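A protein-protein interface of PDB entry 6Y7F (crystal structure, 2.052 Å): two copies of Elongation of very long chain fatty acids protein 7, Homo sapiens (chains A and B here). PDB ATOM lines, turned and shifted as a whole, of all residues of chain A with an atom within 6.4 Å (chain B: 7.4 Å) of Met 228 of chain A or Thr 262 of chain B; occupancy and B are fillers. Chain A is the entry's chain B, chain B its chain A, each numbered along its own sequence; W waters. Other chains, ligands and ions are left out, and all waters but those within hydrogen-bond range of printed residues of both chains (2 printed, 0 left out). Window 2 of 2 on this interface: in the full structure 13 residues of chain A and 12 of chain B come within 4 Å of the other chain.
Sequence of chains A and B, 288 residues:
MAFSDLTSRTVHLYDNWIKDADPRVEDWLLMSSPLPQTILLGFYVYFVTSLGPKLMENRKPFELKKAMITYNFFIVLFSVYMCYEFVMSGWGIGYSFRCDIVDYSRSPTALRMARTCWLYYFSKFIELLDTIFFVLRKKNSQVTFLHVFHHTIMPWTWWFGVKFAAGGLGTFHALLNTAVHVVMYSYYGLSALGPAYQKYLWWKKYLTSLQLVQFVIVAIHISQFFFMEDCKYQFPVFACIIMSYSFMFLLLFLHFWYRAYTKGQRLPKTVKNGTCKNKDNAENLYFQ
No position is printed for both chains.
Of the 9 pairs that touch across the chains among the printed residues, none has its exchanged pair printed and touching as well.
OG1 of Thr 262 of chain B lies within hydrogen-bond range of O of Phe 226 of chain A (2.5 Å).
Water W1 lies within hydrogen-bond range of the side-chain hydroxyl of Tyr 258 of chain B (2.9 Å) and the backbone carbonyl oxygen of Cys 231 of chain A (3.2 Å).
Water W2 bridges the backbone carbonyl oxygen (O) of Thr 262 of chain B (2.9 Å) and the backbone NH (N) of Asp 230 of chain A (3.1 Å).
Met 228 of chain A touches just one residue of chain B: Thr 262.
Thr 262 of chain B touches just these residues of chain A: Phe 226 (2.5 Å), Phe 227 (3.7 Å) and Met 228 (3.4 Å).
Printed residues of chain A within 4 Å of Tyr 258 of chain B: Phe 225 and Phe 226.
Printed residues of chain B within 4 Å of Phe 225 of chain A: Tyr 258.
Printed residues of chain B within 4 Å of Phe 226 of chain A: Leu 254 (3.6 Å), Trp 257 (3.6 Å), Tyr 258 (3.6 Å) and Thr 262 (2.5 Å).
Of the printed residues of chain B, Phe 227 of chain A touches Leu 254 (3.6 Å), Trp 257 (3.3 Å) and Thr 262 (3.7 Å).
Of the printed residues of chain A, Leu 254 of chain B touches Phe 226 and Phe 227.
The nearest residue of chain B that does not touch Met 228 of chain A is Tyr 258 of chain B (5.6 Å).
Hydrophobic or aromatic side chains of chain B that line the printed part of chain A: Leu 254, Trp 257 and Tyr 258.
Printed residues of chain A that touch a printed residue of chain B: Phe 225, Phe 226, Phe 227 and Met 228.
Among the printed residues, 9 pairs touch across the chains.
Among the printed residues, no Asp or Glu carboxylate lies within 4 Å of a Lys or Arg side-chain nitrogen of the other chain.
CZ of Phe 225 of chain A touches OH of Tyr 258 of chain B, at 3.7 Å.
Phe 226 of chain A touches Leu 254 of chain B.
Phe 226 of chain A touches Trp 257 of chain B.
Tyr 258 of chain B touches Phe 226 of chain A.
CZ of Phe 227 of chain A touches CD2 of Leu 254 of chain B, at 3.6 Å.
Phe 227 of chain A touches Trp 257 of chain B (CD1 to NE1, 3.3 Å).
Thr 262 of chain B touches Phe 227 of chain A.
Met 228 of chain A touches Thr 262 of chain B.
The backbone NH (N) of Thr 262 of chain B is in hydrogen-bond range of the backbone carbonyl oxygen (O) of Trp 257 of chain B.
The backbone NH (N) of Lys 263 of chain B is in hydrogen-bond range of the backbone carbonyl oxygen (O) of Tyr 258 of chain B (2.8 Å).
The backbone NH of Cys 99 of chain A sits at hydrogen-bond distance from the side-chain sulfur of Met 228 of chain A.
The side-chain sulfur (SG) of Cys 231 of chain A is disulfide-bonded to the side-chain sulfur (SG) of Cys 99 of chain A (2.1 Å).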
ATOM      1  N   ARG A  98      12.044   5.843  16.676  1.00  0.00           N
ATOM      2  CA  ARG A  98      11.426   6.967  15.983  1.00  0.00           C
ATOM      3  C   ARG A  98      12.490   7.552  15.017  1.00  0.00           C
ATOM      4  O   ARG A  98      12.838   6.861  14.054  1.00  0.00           O
ATOM      5  CB  ARG A  98      10.850   7.966  16.993  1.00  0.00           C
ATOM      6  CG  ARG A  98       9.647   7.410  17.695  1.00  0.00           C
ATOM      7  CD  ARG A  98       9.458   8.030  19.055  1.00  0.00           C
ATOM      8  NE  ARG A  98       8.324   7.438  19.764  1.00  0.00           N
ATOM      9  CZ  ARG A  98       8.379   6.313  20.474  1.00  0.00           C
ATOM     10  NH1 ARG A  98       9.521   5.642  20.582  1.00  0.00           N
ATOM     11  NH2 ARG A  98       7.294   5.856  21.088  1.00  0.00           N
ATOM     12  N   CYS A  99      13.027   8.757  15.259  1.00  0.00           N
ATOM     13  CA  CYS A  99      14.066   9.306  14.395  1.00  0.00           C
ATOM     14  C   CYS A  99      15.429   8.841  14.846  1.00  0.00           C
ATOM     15  O   CYS A  99      16.101   9.541  15.603  1.00  0.00           O
ATOM     16  CB  CYS A  99      14.011  10.830  14.337  1.00  0.00           C
ATOM     17  SG  CYS A  99      15.155  11.559  13.119  1.00  0.00           S
ATOM     18  N   ASP A 100      15.866   7.707  14.351  1.00  0.00           N
ATOM     19  CA  ASP A 100      17.212   7.204  14.626  1.00  0.00           C
ATOM     20  C   ASP A 100      18.066   7.554  13.427  1.00  0.00           C
ATOM     21  O   ASP A 100      17.805   7.069  12.330  1.00  0.00           O
ATOM     22  CB  ASP A 100      17.176   5.706  14.876  1.00  0.00           C
ATOM     23  CG  ASP A 100      16.522   5.372  16.190  1.00  0.00           C
ATOM     24  OD1 ASP A 100      16.953   5.927  17.222  1.00  0.00           O
ATOM     25  OD2 ASP A 100      15.585   4.560  16.194  1.00  0.00           O
ATOM     26  N   LEU A 169      17.272   4.461  11.499  1.00  0.00           N
ATOM     27  CA  LEU A 169      15.925   3.967  11.279  1.00  0.00           C
ATOM     28  C   LEU A 169      15.798   3.054  10.033  1.00  0.00           C
ATOM     29  O   LEU A 169      14.878   2.246   9.973  1.00  0.00           O
ATOM     30  CB  LEU A 169      14.938   5.132  11.231  1.00  0.00           C
ATOM     31  CG  LEU A 169      15.110   6.183  10.145  1.00  0.00           C
ATOM     32  CD1 LEU A 169      14.291   5.818   8.918  1.00  0.00           C
ATOM     33  CD2 LEU A 169      14.586   7.527  10.615  1.00  0.00           C
ATOM     34  N   HIS A 221       6.478   1.388  11.080  1.00  0.00           N
ATOM     35  CA  HIS A 221       7.662   2.034  11.622  1.00  0.00           C
ATOM     36  C   HIS A 221       8.210   3.091  10.651  1.00  0.00           C
ATOM     37  O   HIS A 221       8.469   4.212  11.073  1.00  0.00           O
ATOM     38  CB  HIS A 221       8.758   0.993  11.948  1.00  0.00           C
ATOM     39  CG  HIS A 221      10.086   1.615  12.310  1.00  0.00           C
ATOM     40  ND1 HIS A 221      11.079   1.794  11.363  1.00  0.00           N
ATOM     41  CD2 HIS A 221      10.507   2.127  13.488  1.00  0.00           C
ATOM     42  CE1 HIS A 221      12.087   2.382  11.998  1.00  0.00           C
ATOM     43  NE2 HIS A 221      11.788   2.605  13.278  1.00  0.00           N
ATOM     44  N   ILE A 222       8.435   2.738   9.374  1.00  0.00           N
ATOM     45  CA  ILE A 222       9.006   3.679   8.407  1.00  0.00           C
ATOM     46  C   ILE A 222       8.055   4.828   8.092  1.00  0.00           C
ATOM     47  O   ILE A 222       8.538   5.905   7.742  1.00  0.00           O
ATOM     48  CB  ILE A 222       9.469   2.971   7.113  1.00  0.00           C
ATOM     49  CG1 ILE A 222      10.614   3.736   6.430  1.00  0.00           C
ATOM     50  CG2 ILE A 222       8.328   2.704   6.166  1.00  0.00           C
ATOM     51  CD1 ILE A 222      11.937   3.705   7.243  1.00  0.00           C
ATOM     52  N   SER A 223       6.706   4.625   8.239  1.00  0.00           N
ATOM     53  CA  SER A 223       5.753   5.702   7.969  1.00  0.00           C
ATOM     54  C   SER A 223       5.963   6.897   8.928  1.00  0.00           C
ATOM     55  O   SER A 223       5.609   8.022   8.577  1.00  0.00           O
ATOM     56  CB  SER A 223       4.308   5.200   8.040  1.00  0.00           C
ATOM     57  OG  SER A 223       3.877   5.013   9.378  1.00  0.00           O
ATOM     58  N   GLN A 224       6.548   6.676  10.115  1.00  0.00           N
ATOM     59  CA  GLN A 224       6.804   7.768  11.069  1.00  0.00           C
ATOM     60  C   GLN A 224       7.663   8.871  10.462  1.00  0.00           C
ATOM     61  O   GLN A 224       7.456  10.052  10.783  1.00  0.00           O
ATOM     62  CB  GLN A 224       7.526   7.255  12.315  1.00  0.00           C
ATOM     63  CG  GLN A 224       6.742   6.274  13.153  1.00  0.00           C
ATOM     64  CD  GLN A 224       7.656   5.836  14.266  1.00  0.00           C
ATOM     65  OE1 GLN A 224       7.555   6.323  15.394  1.00  0.00           O
ATOM     66  NE2 GLN A 224       8.615   4.954  13.961  1.00  0.00           N
ATOM     67  N   PHE A 225       8.613   8.488   9.581  1.00  0.00           N
ATOM     68  CA  PHE A 225       9.514   9.407   8.900  1.00  0.00           C
ATOM     69  C   PHE A 225       8.771  10.568   8.216  1.00  0.00           C
ATOM     70  O   PHE A 225       9.207  11.718   8.325  1.00  0.00           O
ATOM     71  CB  PHE A 225      10.381   8.661   7.860  1.00  0.00           C
ATOM     72  CG  PHE A 225      11.299   9.625   7.142  1.00  0.00           C
ATOM     73  CD1 PHE A 225      12.440  10.102   7.756  1.00  0.00           C
ATOM     74  CD2 PHE A 225      10.956  10.146   5.903  1.00  0.00           C
ATOM     75  CE1 PHE A 225      13.238  11.040   7.125  1.00  0.00           C
ATOM     76  CE2 PHE A 225      11.759  11.094   5.283  1.00  0.00           C
ATOM     77  CZ  PHE A 225      12.883  11.533   5.898  1.00  0.00           C
ATOM     78  N   PHE A 226       7.670  10.262   7.502  1.00  0.00           N
ATOM     79  CA  PHE A 226       6.906  11.266   6.778  1.00  0.00           C
ATOM     80  C   PHE A 226       6.272  12.311   7.701  1.00  0.00           C
ATOM     81  O   PHE A 226       5.970  13.415   7.245  1.00  0.00           O
ATOM     82  CB  PHE A 226       5.802  10.576   5.912  1.00  0.00           C
ATOM     83  CG  PHE A 226       6.401   9.558   4.976  1.00  0.00           C
ATOM     84  CD1 PHE A 226       6.984   9.949   3.784  1.00  0.00           C
ATOM     85  CD2 PHE A 226       6.461   8.218   5.328  1.00  0.00           C
ATOM     86  CE1 PHE A 226       7.581   9.017   2.951  1.00  0.00           C
ATOM     87  CE2 PHE A 226       7.084   7.293   4.502  1.00  0.00           C
ATOM     88  CZ  PHE A 226       7.648   7.698   3.325  1.00  0.00           C
ATOM     89  N   PHE A 227       6.045  11.981   8.988  1.00  0.00           N
ATOM     90  CA  PHE A 227       5.360  12.904   9.912  1.00  0.00           C
ATOM     91  C   PHE A 227       6.291  13.597  10.916  1.00  0.00           C
ATOM     92  O   PHE A 227       5.861  14.573  11.552  1.00  0.00           O
ATOM     93  CB  PHE A 227       4.306  12.146  10.719  1.00  0.00           C
ATOM     94  CG  PHE A 227       3.248  11.449   9.899  1.00  0.00           C
ATOM     95  CD1 PHE A 227       2.166  12.143   9.405  1.00  0.00           C
ATOM     96  CD2 PHE A 227       3.308  10.090   9.672  1.00  0.00           C
ATOM     97  CE1 PHE A 227       1.165  11.495   8.676  1.00  0.00           C
ATOM     98  CE2 PHE A 227       2.324   9.453   8.926  1.00  0.00           C
ATOM     99  CZ  PHE A 227       1.264  10.160   8.426  1.00  0.00           C
ATOM    100  N   MET A 228       7.512  13.075  11.116  1.00  0.00           N
ATOM    101  CA  MET A 228       8.397  13.653  12.127  1.00  0.00           C
ATOM    102  C   MET A 228       9.071  14.957  11.695  1.00  0.00           C
ATOM    103  O   MET A 228       9.973  14.938  10.854  1.00  0.00           O
ATOM    104  CB  MET A 228       9.483  12.642  12.550  1.00  0.00           C
ATOM    105  CG  MET A 228       8.904  11.440  13.241  1.00  0.00           C
ATOM    106  SD  MET A 228      10.170  10.308  13.870  1.00  0.00           S
ATOM    107  CE  MET A 228      10.798   9.547  12.361  1.00  0.00           C
ATOM    108  N   GLU A 229       8.677  16.072  12.311  1.00  0.00           N
ATOM    109  CA  GLU A 229       9.351  17.353  12.062  1.00  0.00           C
ATOM    110  C   GLU A 229      10.733  17.336  12.729  1.00  0.00           C
ATOM    111  O   GLU A 229      10.949  16.614  13.714  1.00  0.00           O
ATOM    112  CB  GLU A 229       8.534  18.545  12.562  1.00  0.00           C
ATOM    113  CG  GLU A 229       7.100  18.523  12.084  1.00  0.00           C
ATOM    114  CD  GLU A 229       6.275  19.704  12.553  1.00  0.00           C
ATOM    115  OE1 GLU A 229       6.804  20.839  12.583  1.00  0.00           O
ATOM    116  OE2 GLU A 229       5.086  19.495  12.879  1.00  0.00           O
ATOM    117  N   ASP A 230      11.692  18.032  12.130  1.00  0.00           N
ATOM    118  CA  ASP A 230      13.056  18.118  12.645  1.00  0.00           C
ATOM    119  C   ASP A 230      13.780  16.766  12.715  1.00  0.00           C
ATOM    120  O   ASP A 230      14.758  16.660  13.441  1.00  0.00           O
ATOM    121  CB  ASP A 230      13.088  18.800  14.022  1.00  0.00           C
ATOM    122  N   CYS A 231      13.320  15.735  11.976  1.00  0.00           N
ATOM    123  CA  CYS A 231      14.037  14.461  11.956  1.00  0.00           C
ATOM    124  C   CYS A 231      15.227  14.671  11.028  1.00  0.00           C
ATOM    125  O   CYS A 231      15.065  15.144   9.897  1.00  0.00           O
ATOM    126  CB  CYS A 231      13.133  13.315  11.506  1.00  0.00           C
ATOM    127  SG  CYS A 231      13.945  11.694  11.432  1.00  0.00           S
ATOM    128  N   LYS B 205      -4.865  19.561   7.175  1.00  0.00           N
ATOM    129  CA  LYS B 205      -4.133  18.336   7.525  1.00  0.00           C
ATOM    130  C   LYS B 205      -5.056  17.217   7.958  1.00  0.00           C
ATOM    131  O   LYS B 205      -4.707  16.060   7.755  1.00  0.00           O
ATOM    132  CB  LYS B 205      -3.118  18.604   8.627  1.00  0.00           C
ATOM    133  CG  LYS B 205      -1.958  19.436   8.138  1.00  0.00           C
ATOM    134  CD  LYS B 205      -0.981  19.810   9.243  1.00  0.00           C
ATOM    135  CE  LYS B 205      -0.439  18.637   9.996  1.00  0.00           C
ATOM    136  NZ  LYS B 205       0.471  19.096  11.083  1.00  0.00           N
ATOM    137  N   LEU B 254       1.677   9.995   1.404  1.00  0.00           N
ATOM    138  CA  LEU B 254       2.649  10.147   2.499  1.00  0.00           C
ATOM    139  C   LEU B 254       3.775  11.056   2.022  1.00  0.00           C
ATOM    140  O   LEU B 254       4.179  11.921   2.784  1.00  0.00           O
ATOM    141  CB  LEU B 254       3.185   8.813   3.033  1.00  0.00           C
ATOM    142  CG  LEU B 254       2.167   8.019   3.877  1.00  0.00           C
ATOM    143  CD1 LEU B 254       2.577   6.579   3.983  1.00  0.00           C
ATOM    144  CD2 LEU B 254       1.987   8.632   5.263  1.00  0.00           C
ATOM    145  N   PHE B 256       3.338  13.450  -0.166  1.00  0.00           N
ATOM    146  CA  PHE B 256       2.668  14.742  -0.152  1.00  0.00           C
ATOM    147  C   PHE B 256       2.666  15.302   1.261  1.00  0.00           C
ATOM    148  O   PHE B 256       3.066  16.448   1.437  1.00  0.00           O
ATOM    149  CB  PHE B 256       1.219  14.668  -0.696  1.00  0.00           C
ATOM    150  CG  PHE B 256       0.490  15.988  -0.524  1.00  0.00           C
ATOM    151  CD1 PHE B 256       0.723  17.043  -1.383  1.00  0.00           C
ATOM    152  CD2 PHE B 256      -0.347  16.204   0.563  1.00  0.00           C
ATOM    153  CE1 PHE B 256       0.054  18.259  -1.216  1.00  0.00           C
ATOM    154  CE2 PHE B 256      -0.979  17.434   0.748  1.00  0.00           C
ATOM    155  CZ  PHE B 256      -0.792  18.445  -0.152  1.00  0.00           C
ATOM    156  N   TRP B 257       2.239  14.507   2.278  1.00  0.00           N
ATOM    157  CA  TRP B 257       2.237  14.958   3.675  1.00  0.00           C
ATOM    158  C   TRP B 257       3.627  15.449   4.092  1.00  0.00           C
ATOM    159  O   TRP B 257       3.752  16.504   4.707  1.00  0.00           O
ATOM    160  CB  TRP B 257       1.801  13.834   4.629  1.00  0.00           C
ATOM    161  CG  TRP B 257       1.684  14.298   6.059  1.00  0.00           C
ATOM    162  CD1 TRP B 257       2.687  14.734   6.893  1.00  0.00           C
ATOM    163  CD2 TRP B 257       0.472  14.404   6.800  1.00  0.00           C
ATOM    164  NE1 TRP B 257       2.155  15.150   8.090  1.00  0.00           N
ATOM    165  CE2 TRP B 257       0.795  14.941   8.066  1.00  0.00           C
ATOM    166  CE3 TRP B 257      -0.863  14.088   6.516  1.00  0.00           C
ATOM    167  CZ2 TRP B 257      -0.171  15.154   9.047  1.00  0.00           C
ATOM    168  CZ3 TRP B 257      -1.810  14.305   7.490  1.00  0.00           C
ATOM    169  CH2 TRP B 257      -1.466  14.859   8.728  1.00  0.00           C
ATOM    170  N   TYR B 258       4.653  14.694   3.714  1.00  0.00           N
ATOM    171  CA  TYR B 258       6.030  15.016   4.031  1.00  0.00           C
ATOM    172  C   TYR B 258       6.442  16.374   3.479  1.00  0.00           C
ATOM    173  O   TYR B 258       7.012  17.163   4.249  1.00  0.00           O
ATOM    174  CB  TYR B 258       6.972  13.914   3.511  1.00  0.00           C
ATOM    175  CG  TYR B 258       8.446  14.182   3.773  1.00  0.00           C
ATOM    176  CD1 TYR B 258       8.946  14.226   5.065  1.00  0.00           C
ATOM    177  CD2 TYR B 258       9.337  14.364   2.728  1.00  0.00           C
ATOM    178  CE1 TYR B 258      10.296  14.460   5.311  1.00  0.00           C
ATOM    179  CE2 TYR B 258      10.690  14.594   2.960  1.00  0.00           C
ATOM    180  CZ  TYR B 258      11.166  14.638   4.252  1.00  0.00           C
ATOM    181  OH  TYR B 258      12.494  14.879   4.478  1.00  0.00           O
ATOM    182  N   ARG B 259       6.200  16.671   2.179  1.00  0.00           N
ATOM    183  CA  ARG B 259       6.690  17.951   1.671  1.00  0.00           C
ATOM    184  C   ARG B 259       5.752  19.093   1.971  1.00  0.00           C
ATOM    185  O   ARG B 259       6.246  20.170   2.263  1.00  0.00           O
ATOM    186  CB  ARG B 259       7.096  17.934   0.197  1.00  0.00           C
ATOM    187  CG  ARG B 259       6.104  17.436  -0.738  1.00  0.00           C
ATOM    188  CD  ARG B 259       6.396  18.002  -2.109  1.00  0.00           C
ATOM    189  NE  ARG B 259       5.155  18.001  -2.889  1.00  0.00           N
ATOM    190  CZ  ARG B 259       4.464  19.091  -3.193  1.00  0.00           C
ATOM    191  NH1 ARG B 259       4.925  20.298  -2.856  1.00  0.00           N
ATOM    192  NH2 ARG B 259       3.328  18.991  -3.868  1.00  0.00           N
ATOM    193  N   ALA B 260       4.440  18.863   2.009  1.00  0.00           N
ATOM    194  CA  ALA B 260       3.486  19.920   2.283  1.00  0.00           C
ATOM    195  C   ALA B 260       3.428  20.333   3.767  1.00  0.00           C
ATOM    196  O   ALA B 260       3.201  21.517   4.046  1.00  0.00           O
ATOM    197  CB  ALA B 260       2.092  19.493   1.819  1.00  0.00           C
ATOM    198  N   TYR B 261       3.591  19.382   4.713  1.00  0.00           N
ATOM    199  CA  TYR B 261       3.426  19.713   6.132  1.00  0.00           C
ATOM    200  C   TYR B 261       4.710  19.547   6.922  1.00  0.00           C
ATOM    201  O   TYR B 261       5.123  20.500   7.590  1.00  0.00           O
ATOM    202  CB  TYR B 261       2.302  18.876   6.773  1.00  0.00           C
ATOM    203  CG  TYR B 261       1.003  18.887   5.992  1.00  0.00           C
ATOM    204  CD1 TYR B 261       0.487  20.064   5.481  1.00  0.00           C
ATOM    205  CD2 TYR B 261       0.285  17.721   5.783  1.00  0.00           C
ATOM    206  CE1 TYR B 261      -0.692  20.076   4.743  1.00  0.00           C
ATOM    207  CE2 TYR B 261      -0.916  17.727   5.080  1.00  0.00           C
ATOM    208  CZ  TYR B 261      -1.401  18.907   4.557  1.00  0.00           C
ATOM    209  OH  TYR B 261      -2.584  18.916   3.856  1.00  0.00           O
ATOM    210  N   THR B 262       5.373  18.380   6.831  1.00  0.00           N
ATOM    211  CA  THR B 262       6.606  18.147   7.581  1.00  0.00           C
ATOM    212  C   THR B 262       7.694  19.140   7.128  1.00  0.00           C
ATOM    213  O   THR B 262       8.452  19.663   7.957  1.00  0.00           O
ATOM    214  CB  THR B 262       7.015  16.673   7.435  1.00  0.00           C
ATOM    215  OG1 THR B 262       5.897  15.842   7.791  1.00  0.00           O
ATOM    216  CG2 THR B 262       8.239  16.321   8.240  1.00  0.00           C
ATOM    217  N   LYS B 263       7.770  19.416   5.817  1.00  0.00           N
ATOM    218  CA  LYS B 263       8.746  20.375   5.283  1.00  0.00           C
ATOM    219  C   LYS B 263       8.133  21.775   5.054  1.00  0.00           C
ATOM    220  O   LYS B 263       8.849  22.690   4.652  1.00  0.00           O
ATOM    221  CB  LYS B 263       9.370  19.857   3.983  1.00  0.00           C
ATOM    222  CG  LYS B 263      10.468  18.823   4.215  1.00  0.00           C
ATOM    223  CD  LYS B 263      10.804  18.073   2.943  1.00  0.00           C
ATOM    224  CE  LYS B 263      11.539  18.895   1.916  1.00  0.00           C
ATOM    225  NZ  LYS B 263      11.730  18.141   0.647  1.00  0.00           N
ATOM    226  N   GLY B 264       6.832  21.926   5.319  1.00  0.00           N
ATOM    227  CA  GLY B 264       6.073  23.167   5.231  1.00  0.00           C
ATOM    228  C   GLY B 264       5.930  23.836   3.883  1.00  0.00           C
ATOM    229  O   GLY B 264       5.831  25.059   3.836  1.00  0.00           O
ATOM    230  N   GLN B 265       5.860  23.063   2.786  1.00  0.00           N
ATOM    231  CA  GLN B 265       5.730  23.663   1.461  1.00  0.00           C
ATOM    232  C   GLN B 265       4.309  24.108   1.148  1.00  0.00           C
ATOM    233  O   GLN B 265       4.136  25.047   0.372  1.00  0.00           O
ATOM    234  CB  GLN B 265       6.226  22.719   0.380  1.00  0.00           C
ATOM    235  CG  GLN B 265       7.757  22.705   0.303  1.00  0.00           C
ATOM    236  CD  GLN B 265       8.258  21.752  -0.745  1.00  0.00           C
ATOM    237  OE1 GLN B 265       7.550  21.385  -1.696  1.00  0.00           O
ATOM    238  NE2 GLN B 265       9.503  21.325  -0.586  1.00  0.00           N
ATOM    239  N   LEU B 267       1.505  24.422   3.783  1.00  0.00           N
ATOM    240  CA  LEU B 267       0.816  24.487   5.073  1.00  0.00           C
ATOM    241  C   LEU B 267      -0.510  25.209   4.932  1.00  0.00           C
ATOM    242  O   LEU B 267      -0.638  26.076   4.062  1.00  0.00           O
ATOM    243  CB  LEU B 267       1.694  25.257   6.090  1.00  0.00           C
ATOM    244  CG  LEU B 267       2.972  24.585   6.555  1.00  0.00           C
ATOM    245  CD1 LEU B 267       3.811  25.525   7.399  1.00  0.00           C
ATOM    246  CD2 LEU B 267       2.666  23.290   7.300  1.00  0.00           C
HETATM  247  O   HOH W   1      13.244  14.812   7.261  1.00  0.00           O
HETATM  248  O   HOH W   2      10.941  19.219   9.353  1.00  0.00           O
